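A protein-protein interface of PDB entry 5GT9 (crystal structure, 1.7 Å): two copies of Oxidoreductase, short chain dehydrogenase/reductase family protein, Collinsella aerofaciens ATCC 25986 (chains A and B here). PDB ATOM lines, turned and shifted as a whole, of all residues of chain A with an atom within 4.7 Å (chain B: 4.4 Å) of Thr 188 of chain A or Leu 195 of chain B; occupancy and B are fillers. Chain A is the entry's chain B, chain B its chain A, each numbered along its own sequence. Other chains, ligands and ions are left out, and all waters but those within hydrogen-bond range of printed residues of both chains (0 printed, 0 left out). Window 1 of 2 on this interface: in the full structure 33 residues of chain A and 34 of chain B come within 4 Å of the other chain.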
ATOM      1  N   LEU A 186      28.386  32.672  -3.293  1.00  0.00           N
ATOM      2  CA  LEU A 186      27.938  31.566  -4.107  1.00  0.00           C
ATOM      3  C   LEU A 186      27.964  30.212  -3.395  1.00  0.00           C
ATOM      4  O   LEU A 186      28.804  29.944  -2.564  1.00  0.00           O
ATOM      5  CB  LEU A 186      28.834  31.486  -5.367  1.00  0.00           C
ATOM      6  CG  LEU A 186      28.910  32.737  -6.235  1.00  0.00           C
ATOM      7  CD1 LEU A 186      29.525  32.427  -7.597  1.00  0.00           C
ATOM      8  CD2 LEU A 186      27.662  33.520  -6.367  1.00  0.00           C
ATOM      9  N   GLY A 187      27.015  29.367  -3.783  1.00  0.00           N
ATOM     10  CA  GLY A 187      27.122  27.955  -3.583  1.00  0.00           C
ATOM     11  C   GLY A 187      27.535  27.318  -4.881  1.00  0.00           C
ATOM     12  O   GLY A 187      28.112  27.954  -5.771  1.00  0.00           O
ATOM     13  N   THR A 188      27.187  26.041  -5.010  1.00  0.00           N
ATOM     14  CA  THR A 188      27.515  25.310  -6.235  1.00  0.00           C
ATOM     15  C   THR A 188      27.016  25.980  -7.501  1.00  0.00           C
ATOM     16  O   THR A 188      25.823  26.181  -7.698  1.00  0.00           O
ATOM     17  CB  THR A 188      26.918  23.872  -6.134  1.00  0.00           C
ATOM     18  OG1 THR A 188      27.327  23.332  -4.890  1.00  0.00           O
ATOM     19  CG2 THR A 188      27.482  22.995  -7.215  1.00  0.00           C
ATOM     20  N   THR A 189      27.962  26.191  -8.413  1.00  0.00           N
ATOM     21  CA  THR A 189      27.754  26.991  -9.597  1.00  0.00           C
ATOM     22  C   THR A 189      28.457  26.302 -10.773  1.00  0.00           C
ATOM     23  O   THR A 189      29.547  25.763 -10.589  1.00  0.00           O
ATOM     24  CB  THR A 189      28.398  28.379  -9.397  1.00  0.00           C
ATOM     25  OG1 THR A 189      27.812  28.969  -8.235  1.00  0.00           O
ATOM     26  CG2 THR A 189      28.115  29.289 -10.591  1.00  0.00           C
ATOM     27  N   LEU A 190      27.811  26.303 -11.929  1.00  0.00           N
ATOM     28  CA  LEU A 190      28.321  25.548 -13.111  1.00  0.00           C
ATOM     29  C   LEU A 190      29.520  26.238 -13.760  1.00  0.00           C
ATOM     30  O   LEU A 190      29.359  26.955 -14.738  1.00  0.00           O
ATOM     31  CB  LEU A 190      27.228  25.412 -14.184  1.00  0.00           C
ATOM     32  CG  LEU A 190      25.947  24.662 -13.800  1.00  0.00           C
ATOM     33  CD1 LEU A 190      24.867  24.793 -14.857  1.00  0.00           C
ATOM     34  CD2 LEU A 190      26.250  23.199 -13.526  1.00  0.00           C
ATOM     35  N   LEU A 194      33.691  23.309 -10.923  1.00  0.00           N
ATOM     36  CA  LEU A 194      32.651  22.471 -10.393  1.00  0.00           C
ATOM     37  C   LEU A 194      32.586  21.206 -11.198  1.00  0.00           C
ATOM     38  O   LEU A 194      32.472  20.103 -10.629  1.00  0.00           O
ATOM     39  CB  LEU A 194      31.277  23.132 -10.418  1.00  0.00           C
ATOM     40  CG  LEU A 194      30.184  22.117 -10.066  1.00  0.00           C
ATOM     41  CD1 LEU A 194      30.382  21.684  -8.611  1.00  0.00           C
ATOM     42  CD2 LEU A 194      28.787  22.651 -10.300  1.00  0.00           C
ATOM     43  N   VAL A 207      23.591  16.740  -9.996  1.00  0.00           N
ATOM     44  CA  VAL A 207      24.223  17.970  -9.479  1.00  0.00           C
ATOM     45  C   VAL A 207      23.986  19.115 -10.467  1.00  0.00           C
ATOM     46  O   VAL A 207      23.590  20.175 -10.069  1.00  0.00           O
ATOM     47  CB  VAL A 207      25.720  17.755  -9.211  1.00  0.00           C
ATOM     48  CG1 VAL A 207      26.405  19.067  -8.806  1.00  0.00           C
ATOM     49  CG2 VAL A 207      25.964  16.686  -8.131  1.00  0.00           C
ATOM     50  N   ILE A 210      20.859  21.012  -9.715  1.00  0.00           N
ATOM     51  CA  ILE A 210      20.680  21.802  -8.536  1.00  0.00           C
ATOM     52  C   ILE A 210      21.712  22.929  -8.410  1.00  0.00           C
ATOM     53  O   ILE A 210      21.650  23.704  -7.461  1.00  0.00           O
ATOM     54  CB  ILE A 210      20.605  20.924  -7.264  1.00  0.00           C
ATOM     55  CG1 ILE A 210      21.876  20.096  -7.058  1.00  0.00           C
ATOM     56  CG2 ILE A 210      19.380  20.011  -7.372  1.00  0.00           C
ATOM     57  CD1 ILE A 210      21.778  19.103  -5.897  1.00  0.00           C
ATOM     58  N   ALA A 211      22.640  23.015  -9.361  1.00  0.00           N
ATOM     59  CA  ALA A 211      23.648  24.087  -9.333  1.00  0.00           C
ATOM     60  C   ALA A 211      23.088  25.324  -9.991  1.00  0.00           C
ATOM     61  O   ALA A 211      22.275  25.234 -10.892  1.00  0.00           O
ATOM     62  CB  ALA A 211      24.921  23.649 -10.058  1.00  0.00           C
ATOM     63  N   LEU A 212      23.610  26.498  -9.632  1.00  0.00           N
ATOM     64  CA  LEU A 212      23.219  27.682 -10.334  1.00  0.00           C
ATOM     65  C   LEU A 212      24.104  27.948 -11.553  1.00  0.00           C
ATOM     66  O   LEU A 212      25.221  27.509 -11.569  1.00  0.00           O
ATOM     67  CB  LEU A 212      23.325  28.884  -9.406  1.00  0.00           C
ATOM     68  CG  LEU A 212      22.515  28.729  -8.106  1.00  0.00           C
ATOM     69  CD1 LEU A 212      22.556  30.029  -7.358  1.00  0.00           C
ATOM     70  CD2 LEU A 212      21.088  28.320  -8.402  1.00  0.00           C
ATOM     71  N   LEU B 190      23.742  15.017  -0.566  1.00  0.00           N
ATOM     72  CA  LEU B 190      24.307  16.293  -1.043  1.00  0.00           C
ATOM     73  C   LEU B 190      23.289  17.403  -1.002  1.00  0.00           C
ATOM     74  O   LEU B 190      22.501  17.597  -1.941  1.00  0.00           O
ATOM     75  CB  LEU B 190      24.809  16.167  -2.465  1.00  0.00           C
ATOM     76  CG  LEU B 190      25.940  15.129  -2.611  1.00  0.00           C
ATOM     77  CD1 LEU B 190      26.166  14.771  -4.065  1.00  0.00           C
ATOM     78  CD2 LEU B 190      27.214  15.742  -2.004  1.00  0.00           C
ATOM     79  N   THR B 191      23.356  18.166   0.056  1.00  0.00           N
ATOM     80  CA  THR B 191      22.471  19.268   0.304  1.00  0.00           C
ATOM     81  C   THR B 191      23.237  20.527  -0.046  1.00  0.00           C
ATOM     82  O   THR B 191      24.416  20.487  -0.422  1.00  0.00           O
ATOM     83  CB  THR B 191      21.981  19.223   1.768  1.00  0.00           C
ATOM     84  OG1 THR B 191      23.110  19.138   2.654  1.00  0.00           O
ATOM     85  CG2 THR B 191      21.117  17.991   1.988  1.00  0.00           C
ATOM     86  N   PRO B 192      22.566  21.691   0.004  1.00  0.00           N
ATOM     87  CA  PRO B 192      23.199  22.845  -0.659  1.00  0.00           C
ATOM     88  C   PRO B 192      24.537  23.276  -0.037  1.00  0.00           C
ATOM     89  O   PRO B 192      25.448  23.609  -0.769  1.00  0.00           O
ATOM     90  CB  PRO B 192      22.154  23.959  -0.503  1.00  0.00           C
ATOM     91  CG  PRO B 192      20.837  23.182  -0.503  1.00  0.00           C
ATOM     92  CD  PRO B 192      21.138  21.913   0.290  1.00  0.00           C
ATOM     93  N   SER B 193      24.634  23.280   1.290  1.00  0.00           N
ATOM     94  CA  SER B 193      25.918  23.674   1.936  1.00  0.00           C
ATOM     95  C   SER B 193      27.027  22.655   1.755  1.00  0.00           C
ATOM     96  O   SER B 193      28.176  22.977   1.482  1.00  0.00           O
ATOM     97  CB  SER B 193      25.694  23.945   3.433  1.00  0.00           C
ATOM     98  OG  SER B 193      24.829  25.039   3.633  1.00  0.00           O
ATOM     99  N   LEU B 194      26.663  21.397   1.864  1.00  0.00           N
ATOM    100  CA  LEU B 194      27.658  20.334   1.722  1.00  0.00           C
ATOM    101  C   LEU B 194      28.228  20.300   0.340  1.00  0.00           C
ATOM    102  O   LEU B 194      29.456  20.189   0.142  1.00  0.00           O
ATOM    103  CB  LEU B 194      27.034  19.008   2.072  1.00  0.00           C
ATOM    104  CG  LEU B 194      27.973  17.895   2.408  1.00  0.00           C
ATOM    105  CD1 LEU B 194      29.046  18.322   3.420  1.00  0.00           C
ATOM    106  CD2 LEU B 194      27.082  16.792   2.905  1.00  0.00           C
ATOM    107  N   LEU B 195      27.361  20.508  -0.655  1.00  0.00           N
ATOM    108  CA  LEU B 195      27.825  20.568  -2.007  1.00  0.00           C
ATOM    109  C   LEU B 195      28.875  21.621  -2.199  1.00  0.00           C
ATOM    110  O   LEU B 195      29.786  21.449  -2.992  1.00  0.00           O
ATOM    111  CB  LEU B 195      26.693  20.812  -3.005  1.00  0.00           C
ATOM    112  CG  LEU B 195      26.133  19.591  -3.725  1.00  0.00           C
ATOM    113  CD1 LEU B 195      24.979  20.014  -4.622  1.00  0.00           C
ATOM    114  CD2 LEU B 195      27.180  18.832  -4.552  1.00  0.00           C
ATOM    115  N   SER B 196      28.745  22.748  -1.509  1.00  0.00           N
ATOM    116  CA  SER B 196      29.716  23.824  -1.737  1.00  0.00           C
ATOM    117  C   SER B 196      31.056  23.572  -1.075  1.00  0.00           C
ATOM    118  O   SER B 196      31.962  24.398  -1.155  1.00  0.00           O
ATOM    119  CB  SER B 196      29.116  25.155  -1.261  1.00  0.00           C
ATOM    120  OG  SER B 196      27.762  25.156  -1.569  1.00  0.00           O
ATOM    121  N   ASN B 197      31.183  22.451  -0.362  1.00  0.00           N
ATOM    122  CA  ASN B 197      32.471  21.998   0.174  1.00  0.00           C
ATOM    123  C   ASN B 197      32.993  20.795  -0.561  1.00  0.00           C
ATOM    124  O   ASN B 197      33.704  20.023   0.032  1.00  0.00           O
ATOM    125  CB  ASN B 197      32.351  21.639   1.681  1.00  0.00           C
ATOM    126  CG  ASN B 197      33.686  21.610   2.410  1.00  0.00           C
ATOM    127  OD1 ASN B 197      34.623  22.193   1.974  1.00  0.00           O
ATOM    128  ND2 ASN B 197      33.780  20.849   3.518  1.00  0.00           N
ATOM    129  N   LEU B 198      32.719  20.683  -1.858  1.00  0.00           N
ATOM    130  CA  LEU B 198      33.449  19.734  -2.693  1.00  0.00           C
ATOM    131  C   LEU B 198      34.907  20.108  -2.892  1.00  0.00           C
ATOM    132  O   LEU B 198      35.208  21.243  -3.227  1.00  0.00           O
ATOM    133  CB  LEU B 198      32.834  19.623  -4.066  1.00  0.00           C
ATOM    134  CG  LEU B 198      31.524  18.881  -4.080  1.00  0.00           C
ATOM    135  CD1 LEU B 198      30.791  19.152  -5.394  1.00  0.00           C
ATOM    136  CD2 LEU B 198      31.749  17.393  -3.867  1.00  0.00           C
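Ser 196 of chain B touches Gly 187 of chain A (OG to CA, 3.5 Å).
Leu 195 of chain B touches Thr 188 of chain A (CB to OG1, 3.2 Å).
OG of Ser 196 of chain B touches N of Thr 188 of chain A, 3.6 Å away.
Leu 195 of chain B touches Ile 210 of chain A (CD1 to CD1, 3.6 Å).
The backbone NH (N) of Leu 212 of chain A sits at hydrogen-bond distance from the backbone carbonyl oxygen (O) of Thr 188 of chain A, 3.0 Å away.
The backbone carbonyl oxygen (O) of Gly 187 of chain A sits at hydrogen-bond distance from the side-chain hydroxyl (OG1) of Thr 189 of chain A (2.7 Å).
The side-chain hydroxyl (OG) of Ser 196 of chain B sits at hydrogen-bond distance from the backbone carbonyl oxygen (O) of Pro 192 of chain B, 2.9 Å away.
Of chain B, only Leu 195 (3.2 Å) and Ser 196 (3.6 Å) come within 4 Å of Thr 188 of chain A.
Leu 195 of chain B touches just these residues of chain A: Thr 188 (3.2 Å) and Ile 210 (3.6 Å).
Printed residues of chain B within 4 Å of Ile 210 of chain A: Leu 195 (3.6 Å).
Printed residues of chain A within 4 Å of Ser 196 of chain B: Gly 187 and Thr 188.
Printed residues of chain B within 4 Å of Gly 187 of chain A: Ser 196 (3.5 Å).
Thr 189 of chain A touches none of the printed residues of chain B.
Asn 197 of chain B touches none of the printed residues of chain A.
The nearest printed residue of chain B that does not touch Thr 188 of chain A is Pro 192 of chain B (4.5 Å).
The nearest residue of chain A that does not touch Leu 195 of chain B is Val 207 of chain A (4.3 Å).
Of the 10 printed residues of chain A, 3 touch a printed residue of chain B.
Hydrophobic or aromatic side chains of chain A that line the printed part of chain B: Ile 210.
Printed residues of chain B that touch a printed residue of chain A: Leu 195 and Ser 196.
Hydrophobic or aromatic side chains of chain B that line the printed part of chain A: Leu 195.
Positions printed for both chains: 190 and 194.
Of the 4 pairs that touch across the chains among the printed residues, none has its exchanged pair printed and touching as well.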
